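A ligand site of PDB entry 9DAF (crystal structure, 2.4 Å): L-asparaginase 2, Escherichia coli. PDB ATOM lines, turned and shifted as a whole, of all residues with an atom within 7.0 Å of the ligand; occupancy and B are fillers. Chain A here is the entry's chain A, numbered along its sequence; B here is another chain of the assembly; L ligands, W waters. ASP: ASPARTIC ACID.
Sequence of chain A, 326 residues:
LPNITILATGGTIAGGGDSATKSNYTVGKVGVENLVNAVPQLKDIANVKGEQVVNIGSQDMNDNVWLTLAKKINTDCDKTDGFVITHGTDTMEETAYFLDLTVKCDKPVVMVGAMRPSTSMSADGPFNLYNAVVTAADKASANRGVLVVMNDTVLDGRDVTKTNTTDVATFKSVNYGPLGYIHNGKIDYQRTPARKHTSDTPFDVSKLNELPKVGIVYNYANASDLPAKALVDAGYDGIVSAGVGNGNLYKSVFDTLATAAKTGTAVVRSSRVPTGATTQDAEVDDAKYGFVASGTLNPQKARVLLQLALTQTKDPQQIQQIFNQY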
ATOM      1  N   GLY A  10     -18.536  22.434 -21.164  1.00  0.00           N
ATOM      2  CA  GLY A  10     -19.150  23.476 -21.958  1.00  0.00           C
ATOM      3  C   GLY A  10     -20.331  22.930 -22.734  1.00  0.00           C
ATOM      4  O   GLY A  10     -20.993  22.011 -22.269  1.00  0.00           O
ATOM      5  N   GLY A  11     -20.582  23.515 -23.890  1.00  0.00           N
ATOM      6  CA  GLY A  11     -21.594  23.048 -24.826  1.00  0.00           C
ATOM      7  C   GLY A  11     -22.785  24.010 -24.921  1.00  0.00           C
ATOM      8  O   GLY A  11     -22.921  24.946 -24.136  1.00  0.00           O
ATOM      9  N   THR A  12     -23.648  23.755 -25.896  1.00  0.00           N
ATOM     10  CA  THR A  12     -24.973  24.352 -25.897  1.00  0.00           C
ATOM     11  C   THR A  12     -25.668  23.986 -24.590  1.00  0.00           C
ATOM     12  O   THR A  12     -26.551  24.718 -24.140  1.00  0.00           O
ATOM     13  CB  THR A  12     -25.792  23.885 -27.111  1.00  0.00           C
ATOM     14  OG1 THR A  12     -25.107  24.352 -28.272  1.00  0.00           O
ATOM     15  CG2 THR A  12     -27.206  24.428 -27.111  1.00  0.00           C
ATOM     16  N   ILE A  13     -25.282  22.843 -23.981  1.00  0.00           N
ATOM     17  CA  ILE A  13     -26.021  22.336 -22.841  1.00  0.00           C
ATOM     18  C   ILE A  13     -25.915  23.359 -21.727  1.00  0.00           C
ATOM     19  O   ILE A  13     -26.881  23.532 -20.979  1.00  0.00           O
ATOM     20  CB  ILE A  13     -25.575  20.945 -22.368  1.00  0.00           C
ATOM     21  CG1 ILE A  13     -26.600  20.368 -21.364  1.00  0.00           C
ATOM     22  CG2 ILE A  13     -24.145  20.956 -21.794  1.00  0.00           C
ATOM     23  CD1 ILE A  13     -26.303  18.979 -20.816  1.00  0.00           C
ATOM     24  N   TYR A  25     -27.294  31.867 -30.046  1.00  0.00           N
ATOM     25  CA  TYR A  25     -26.847  31.509 -28.702  1.00  0.00           C
ATOM     26  C   TYR A  25     -25.318  31.568 -28.621  1.00  0.00           C
ATOM     27  O   TYR A  25     -24.631  31.523 -29.637  1.00  0.00           O
ATOM     28  CB  TYR A  25     -27.419  30.142 -28.309  1.00  0.00           C
ATOM     29  CG  TYR A  25     -26.978  28.911 -29.104  1.00  0.00           C
ATOM     30  CD1 TYR A  25     -27.626  28.517 -30.276  1.00  0.00           C
ATOM     31  CD2 TYR A  25     -25.949  28.101 -28.650  1.00  0.00           C
ATOM     32  CE1 TYR A  25     -27.248  27.387 -30.982  1.00  0.00           C
ATOM     33  CE2 TYR A  25     -25.556  26.965 -29.341  1.00  0.00           C
ATOM     34  CZ  TYR A  25     -26.209  26.605 -30.508  1.00  0.00           C
ATOM     35  OH  TYR A  25     -25.781  25.462 -31.152  1.00  0.00           O
ATOM     36  N   VAL A  27     -22.192  29.495 -26.377  1.00  0.00           N
ATOM     37  CA  VAL A  27     -21.964  28.230 -25.701  1.00  0.00           C
ATOM     38  C   VAL A  27     -20.851  28.407 -24.663  1.00  0.00           C
ATOM     39  O   VAL A  27     -20.024  29.302 -24.800  1.00  0.00           O
ATOM     40  CB  VAL A  27     -21.630  27.079 -26.670  1.00  0.00           C
ATOM     41  CG1 VAL A  27     -22.759  26.845 -27.662  1.00  0.00           C
ATOM     42  CG2 VAL A  27     -20.309  27.301 -27.406  1.00  0.00           C
ATOM     43  N   GLY A  28     -20.845  27.520 -23.663  1.00  0.00           N
ATOM     44  CA  GLY A  28     -19.850  27.517 -22.607  1.00  0.00           C
ATOM     45  C   GLY A  28     -19.941  28.733 -21.674  1.00  0.00           C
ATOM     46  O   GLY A  28     -18.906  29.263 -21.259  1.00  0.00           O
ATOM     47  N   ILE A  56     -16.069  25.494 -22.828  1.00  0.00           N
ATOM     48  CA  ILE A  56     -15.879  25.834 -24.235  1.00  0.00           C
ATOM     49  C   ILE A  56     -16.944  25.179 -25.109  1.00  0.00           C
ATOM     50  O   ILE A  56     -17.528  24.153 -24.760  1.00  0.00           O
ATOM     51  CB  ILE A  56     -14.469  25.427 -24.704  1.00  0.00           C
ATOM     52  CG1 ILE A  56     -14.229  23.905 -24.591  1.00  0.00           C
ATOM     53  CG2 ILE A  56     -13.398  26.220 -23.958  1.00  0.00           C
ATOM     54  CD1 ILE A  56     -12.964  23.390 -25.272  1.00  0.00           C
ATOM     55  N   GLY A  57     -17.170  25.758 -26.285  1.00  0.00           N
ATOM     56  CA  GLY A  57     -17.858  25.059 -27.348  1.00  0.00           C
ATOM     57  C   GLY A  57     -16.975  23.900 -27.826  1.00  0.00           C
ATOM     58  O   GLY A  57     -15.759  24.029 -27.854  1.00  0.00           O
ATOM     59  N   SER A  58     -17.586  22.774 -28.171  1.00  0.00           N
ATOM     60  CA  SER A  58     -16.807  21.566 -28.468  1.00  0.00           C
ATOM     61  C   SER A  58     -16.192  21.627 -29.867  1.00  0.00           C
ATOM     62  O   SER A  58     -15.433  20.725 -30.210  1.00  0.00           O
ATOM     63  CB  SER A  58     -17.621  20.311 -28.276  1.00  0.00           C
ATOM     64  OG  SER A  58     -18.621  20.180 -29.276  1.00  0.00           O
ATOM     65  N   GLN A  59     -16.487  22.669 -30.655  1.00  0.00           N
ATOM     66  CA  GLN A  59     -15.751  22.895 -31.893  1.00  0.00           C
ATOM     67  C   GLN A  59     -14.295  23.215 -31.582  1.00  0.00           C
ATOM     68  O   GLN A  59     -13.424  23.076 -32.452  1.00  0.00           O
ATOM     69  CB  GLN A  59     -16.344  24.009 -32.751  1.00  0.00           C
ATOM     70  CG  GLN A  59     -16.419  25.377 -32.073  1.00  0.00           C
ATOM     71  CD  GLN A  59     -17.708  25.575 -31.305  1.00  0.00           C
ATOM     72  OE1 GLN A  59     -18.170  24.714 -30.558  1.00  0.00           O
ATOM     73  NE2 GLN A  59     -18.344  26.725 -31.504  1.00  0.00           N
ATOM     74  N   ASP A  60     -14.014  23.619 -30.333  1.00  0.00           N
ATOM     75  CA  ASP A  60     -12.684  24.002 -29.933  1.00  0.00           C
ATOM     76  C   ASP A  60     -12.037  22.929 -29.054  1.00  0.00           C
ATOM     77  O   ASP A  60     -10.959  23.144 -28.499  1.00  0.00           O
ATOM     78  CB  ASP A  60     -12.734  25.354 -29.240  1.00  0.00           C
ATOM     79  CG  ASP A  60     -12.887  26.565 -30.146  1.00  0.00           C
ATOM     80  OD1 ASP A  60     -12.787  26.424 -31.387  1.00  0.00           O
ATOM     81  OD2 ASP A  60     -13.047  27.684 -29.579  1.00  0.00           O
ATOM     82  N   HIS A  87     -21.045  18.390 -22.306  1.00  0.00           N
ATOM     83  CA  HIS A  87     -20.173  18.565 -23.463  1.00  0.00           C
ATOM     84  C   HIS A  87     -21.034  19.070 -24.619  1.00  0.00           C
ATOM     85  O   HIS A  87     -22.222  18.760 -24.734  1.00  0.00           O
ATOM     86  CB  HIS A  87     -19.429  17.245 -23.712  1.00  0.00           C
ATOM     87  CG  HIS A  87     -18.364  17.210 -24.764  1.00  0.00           C
ATOM     88  ND1 HIS A  87     -17.049  16.967 -24.422  1.00  0.00           N
ATOM     89  CD2 HIS A  87     -18.377  17.268 -26.108  1.00  0.00           C
ATOM     90  CE1 HIS A  87     -16.297  16.949 -25.512  1.00  0.00           C
ATOM     91  NE2 HIS A  87     -17.076  17.135 -26.552  1.00  0.00           N
ATOM     92  N   GLY A  88     -20.444  19.900 -25.470  1.00  0.00           N
ATOM     93  CA  GLY A  88     -21.072  20.221 -26.743  1.00  0.00           C
ATOM     94  C   GLY A  88     -21.243  18.979 -27.606  1.00  0.00           C
ATOM     95  O   GLY A  88     -20.532  17.988 -27.449  1.00  0.00           O
ATOM     96  N   THR A  89     -22.157  19.074 -28.564  1.00  0.00           N
ATOM     97  CA  THR A  89     -22.531  17.949 -29.390  1.00  0.00           C
ATOM     98  C   THR A  89     -21.655  17.831 -30.633  1.00  0.00           C
ATOM     99  O   THR A  89     -21.663  16.781 -31.275  1.00  0.00           O
ATOM    100  CB  THR A  89     -24.007  18.089 -29.764  1.00  0.00           C
ATOM    101  OG1 THR A  89     -24.187  19.314 -30.476  1.00  0.00           O
ATOM    102  CG2 THR A  89     -24.915  18.023 -28.542  1.00  0.00           C
ATOM    103  N   ASP A  90     -20.972  18.912 -31.017  1.00  0.00           N
ATOM    104  CA  ASP A  90     -20.228  18.981 -32.260  1.00  0.00           C
ATOM    105  C   ASP A  90     -19.127  17.915 -32.390  1.00  0.00           C
ATOM    106  O   ASP A  90     -19.014  17.321 -33.467  1.00  0.00           O
ATOM    107  CB  ASP A  90     -19.682  20.384 -32.484  1.00  0.00           C
ATOM    108  CG  ASP A  90     -20.746  21.428 -32.845  1.00  0.00           C
ATOM    109  OD1 ASP A  90     -21.959  21.094 -32.939  1.00  0.00           O
ATOM    110  OD2 ASP A  90     -20.327  22.566 -33.081  1.00  0.00           O
ATOM    111  N   THR A  91     -18.369  17.676 -31.296  1.00  0.00           N
ATOM    112  CA  THR A  91     -17.294  16.695 -31.271  1.00  0.00           C
ATOM    113  C   THR A  91     -17.464  15.703 -30.102  1.00  0.00           C
ATOM    114  O   THR A  91     -16.525  14.970 -29.777  1.00  0.00           O
ATOM    115  CB  THR A  91     -15.919  17.369 -31.191  1.00  0.00           C
ATOM    116  OG1 THR A  91     -15.787  18.111 -29.985  1.00  0.00           O
ATOM    117  CG2 THR A  91     -15.653  18.324 -32.332  1.00  0.00           C
ATOM    118  N   MET A  92     -18.669  15.619 -29.530  1.00  0.00           N
ATOM    119  CA  MET A  92     -18.958  14.647 -28.497  1.00  0.00           C
ATOM    120  C   MET A  92     -18.590  13.254 -28.996  1.00  0.00           C
ATOM    121  O   MET A  92     -18.127  12.422 -28.259  1.00  0.00           O
ATOM    122  CB  MET A  92     -20.455  14.597 -28.138  1.00  0.00           C
ATOM    123  CG  MET A  92     -20.770  13.718 -26.926  1.00  0.00           C
ATOM    124  SD  MET A  92     -22.361  14.047 -26.111  1.00  0.00           S
ATOM    125  CE  MET A  92     -22.204  15.748 -25.570  1.00  0.00           C
ATOM    126  N   GLY A 113     -25.114  16.010 -23.949  1.00  0.00           N
ATOM    127  CA  GLY A 113     -25.275  17.419 -24.258  1.00  0.00           C
ATOM    128  C   GLY A 113     -26.725  17.778 -24.606  1.00  0.00           C
ATOM    129  O   GLY A 113     -27.678  17.140 -24.182  1.00  0.00           O
ATOM    130  N   ALA A 114     -26.884  18.851 -25.384  1.00  0.00           N
ATOM    131  CA  ALA A 114     -28.202  19.362 -25.710  1.00  0.00           C
ATOM    132  C   ALA A 114     -28.143  20.064 -27.059  1.00  0.00           C
ATOM    133  O   ALA A 114     -27.247  20.862 -27.268  1.00  0.00           O
ATOM    134  CB  ALA A 114     -28.653  20.319 -24.630  1.00  0.00           C
ATOM    135  N   MET A 115     -29.121  19.792 -27.921  1.00  0.00           N
ATOM    136  CA  MET A 115     -29.170  20.456 -29.210  1.00  0.00           C
ATOM    137  C   MET A 115     -29.741  21.879 -29.116  1.00  0.00           C
ATOM    138  O   MET A 115     -29.508  22.666 -30.036  1.00  0.00           O
ATOM    139  CB  MET A 115     -29.952  19.596 -30.205  1.00  0.00           C
ATOM    140  CG  MET A 115     -29.176  18.343 -30.634  1.00  0.00           C
ATOM    141  SD  MET A 115     -27.572  18.725 -31.370  1.00  0.00           S
ATOM    142  CE  MET A 115     -28.131  19.340 -32.959  1.00  0.00           C
ATOM    143  N   ARG A 116     -30.501  22.183 -28.051  1.00  0.00           N
ATOM    144  CA  ARG A 116     -31.120  23.487 -27.846  1.00  0.00           C
ATOM    145  C   ARG A 116     -30.588  24.127 -26.582  1.00  0.00           C
ATOM    146  O   ARG A 116     -30.467  23.456 -25.566  1.00  0.00           O
ATOM    147  CB  ARG A 116     -32.634  23.458 -27.638  1.00  0.00           C
ATOM    148  CG  ARG A 116     -33.366  22.879 -28.845  1.00  0.00           C
ATOM    149  CD  ARG A 116     -34.875  22.805 -28.609  1.00  0.00           C
ATOM    150  NE  ARG A 116     -35.563  22.116 -29.706  1.00  0.00           N
ATOM    151  CZ  ARG A 116     -36.708  21.456 -29.565  1.00  0.00           C
ATOM    152  NH1 ARG A 116     -37.240  21.298 -28.381  1.00  0.00           N
ATOM    153  NH2 ARG A 116     -37.315  20.919 -30.611  1.00  0.00           N
ATOM    154  N   LYS A 162     -23.248  12.052 -34.748  1.00  0.00           N
ATOM    155  CA  LYS A 162     -24.228  13.100 -34.930  1.00  0.00           C
ATOM    156  C   LYS A 162     -24.693  12.970 -36.381  1.00  0.00           C
ATOM    157  O   LYS A 162     -23.854  13.062 -37.253  1.00  0.00           O
ATOM    158  CB  LYS A 162     -23.593  14.454 -34.580  1.00  0.00           C
ATOM    159  CG  LYS A 162     -24.563  15.625 -34.473  1.00  0.00           C
ATOM    160  CD  LYS A 162     -23.941  16.965 -34.083  1.00  0.00           C
ATOM    161  CE  LYS A 162     -24.943  18.067 -33.977  1.00  0.00           C
ATOM    162  NZ  LYS A 162     -24.355  19.321 -33.484  1.00  0.00           N
ATOM    163  N   THR A 165     -27.818  18.199 -38.218  1.00  0.00           N
ATOM    164  CA  THR A 165     -27.237  19.436 -37.693  1.00  0.00           C
ATOM    165  C   THR A 165     -28.073  20.095 -36.591  1.00  0.00           C
ATOM    166  O   THR A 165     -27.517  20.889 -35.855  1.00  0.00           O
ATOM    167  CB  THR A 165     -27.039  20.471 -38.807  1.00  0.00           C
ATOM    168  OG1 THR A 165     -28.314  20.790 -39.340  1.00  0.00           O
ATOM    169  CG2 THR A 165     -26.111  20.017 -39.919  1.00  0.00           C
ATOM    170  N   VAL B 244     -18.094  21.128 -38.123  1.00  0.00           N
ATOM    171  CA  VAL B 244     -18.625  20.229 -37.116  1.00  0.00           C
ATOM    172  C   VAL B 244     -19.984  20.784 -36.673  1.00  0.00           C
ATOM    173  O   VAL B 244     -20.166  22.003 -36.642  1.00  0.00           O
ATOM    174  CB  VAL B 244     -17.646  20.099 -35.931  1.00  0.00           C
ATOM    175  CG1 VAL B 244     -16.363  19.350 -36.258  1.00  0.00           C
ATOM    176  CG2 VAL B 244     -17.353  21.438 -35.318  1.00  0.00           C
ATOM    177  N   GLY B 245     -20.951  19.897 -36.416  1.00  0.00           N
ATOM    178  CA  GLY B 245     -22.332  20.334 -36.191  1.00  0.00           C
ATOM    179  C   GLY B 245     -22.866  21.299 -37.255  1.00  0.00           C
ATOM    180  O   GLY B 245     -22.748  21.036 -38.456  1.00  0.00           O
ATOM    181  N   ASN B 246     -23.480  22.402 -36.808  1.00  0.00           N
ATOM    182  CA  ASN B 246     -24.089  23.404 -37.688  1.00  0.00           C
ATOM    183  C   ASN B 246     -23.001  24.323 -38.270  1.00  0.00           C
ATOM    184  O   ASN B 246     -22.950  25.506 -37.961  1.00  0.00           O
ATOM    185  CB  ASN B 246     -25.162  24.166 -36.918  1.00  0.00           C
ATOM    186  CG  ASN B 246     -26.094  24.980 -37.814  1.00  0.00           C
ATOM    187  OD1 ASN B 246     -25.947  25.010 -39.041  1.00  0.00           O
ATOM    188  ND2 ASN B 246     -27.095  25.614 -37.224  1.00  0.00           N
ATOM    189  N   ASN B 248     -19.843  24.654 -37.696  1.00  0.00           N
ATOM    190  CA  ASN B 248     -18.893  25.287 -36.790  1.00  0.00           C
ATOM    191  C   ASN B 248     -17.452  24.903 -37.150  1.00  0.00           C
ATOM    192  O   ASN B 248     -17.203  23.924 -37.848  1.00  0.00           O
ATOM    193  CB  ASN B 248     -19.223  25.007 -35.334  1.00  0.00           C
ATOM    194  CG  ASN B 248     -20.505  25.693 -34.902  1.00  0.00           C
ATOM    195  OD1 ASN B 248     -20.681  26.901 -35.139  1.00  0.00           O
ATOM    196  ND2 ASN B 248     -21.412  24.944 -34.281  1.00  0.00           N
ATOM    197  N   GLU B 283     -24.225  30.165 -34.379  1.00  0.00           N
ATOM    198  CA  GLU B 283     -23.094  30.555 -33.556  1.00  0.00           C
ATOM    199  C   GLU B 283     -22.151  31.453 -34.342  1.00  0.00           C
ATOM    200  O   GLU B 283     -21.398  32.215 -33.751  1.00  0.00           O
ATOM    201  CB  GLU B 283     -22.277  29.366 -33.035  1.00  0.00           C
ATOM    202  CG  GLU B 283     -23.031  28.548 -32.001  1.00  0.00           C
ATOM    203  CD  GLU B 283     -22.287  27.337 -31.443  1.00  0.00           C
ATOM    204  OE1 GLU B 283     -21.201  27.567 -30.820  1.00  0.00           O
ATOM    205  OE2 GLU B 283     -22.805  26.182 -31.585  1.00  0.00           O
HETATM  206  N   ASP L   1     -21.072  24.418 -30.636  1.00  0.00           N
HETATM  207  CA  ASP L   1     -21.855  23.576 -29.668  1.00  0.00           C
HETATM  208  C   ASP L   1     -20.860  22.547 -29.162  1.00  0.00           C
HETATM  209  O   ASP L   1     -20.894  21.420 -29.712  1.00  0.00           O
HETATM  210  CB  ASP L   1     -23.111  22.951 -30.265  1.00  0.00           C
HETATM  211  CG  ASP L   1     -23.934  22.063 -29.346  1.00  0.00           C
HETATM  212  OD1 ASP L   1     -23.473  21.814 -28.206  1.00  0.00           O
HETATM  213  OD2 ASP L   1     -25.073  21.637 -29.735  1.00  0.00           O
HETATM  214  OXT ASP L   1     -20.053  22.959 -28.305  1.00  0.00           O
HETATM  215  O   HOH W   1     -24.069  20.404 -25.624  1.00  0.00           O
HETATM  216  O   HOH W   2     -26.971  23.035 -31.440  1.00  0.00           O
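N of the ligand sits at hydrogen-bond distance from OE1 of Gln 59 (2.9 Å). The backbone NH (N) of Thr 89 is in hydrogen-bond range of an oxygen (O) of the ligand. The side-chain hydroxyl (OG1) of Thr 12 sits close to an oxygen (OD1) of the ligand (3.0 Å). OD1 of the ligand lies within hydrogen-bond range of N of Thr 12, 3.0 Å away. An oxygen (OXT) of the ligand is in hydrogen-bond range of the backbone NH of Ser 58 (2.5 Å). OD2 of the ligand is in hydrogen-bond range of OG1 of Thr 89 (2.6 Å). A nitrogen (N) of the ligand lies within salt-bridge range of the side-chain carboxylate (OE2) of Glu 283 of chain B. The side-chain hydroxyl (OG) of Ser 58 lies within hydrogen-bond range of an oxygen (O) of the ligand. The side-chain carboxylate of Asp 90 is in salt-bridge range of a nitrogen (N) of the ligand, 3.2 Å away. N of Asp 90 sits at hydrogen-bond distance from O of the ligand.
The side-chain hydroxyl of Ser 58 is in hydrogen-bond range of the backbone NH of Asp 90, 3.2 Å away. The backbone carbonyl oxygen (O) of Ile 56 lies within hydrogen-bond range of the backbone NH (N) of Gly 11, 3.2 Å away. OG1 of Thr 12 sits close to OH of Tyr 25 (3.2 Å). OG1 of Thr 89 is in hydrogen-bond range of NZ of Lys 162, 3.0 Å away. The side-chain hydroxyl (OG1) of Thr 89 is in hydrogen-bond range of the side-chain sulfur (SD) of Met 115, at 3.6 Å. ND2 of Asn 248 of chain B lies within hydrogen-bond range of OD2 of Asp 90. The side-chain hydroxyl of Ser 58 sits close to the backbone carbonyl oxygen of Gly 88, at 3.4 Å. OD1 of Asp 90 is in salt-bridge range of NZ of Lys 162 (3.0 Å).
An oxygen (OD2) of the ligand lies close to the backbone carbonyl oxygen (O) of Ala 114, at 3.4 Å. Merely in contact with the ligand: Gly 57 (3.2 Å), Gly 88 (3.2 Å), Asn 248 of chain B (3.7 Å), Tyr 25 (3.8 Å), Gly 11 (3.8 Å) and Val 27 (3.9 Å). Hydrophobic or aromatic side chains within 4 Å of the ligand: Val 27.
Water W2 lies within hydrogen-bond range of OH of Tyr 25, OD2 of the ligand and O of Met 115.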
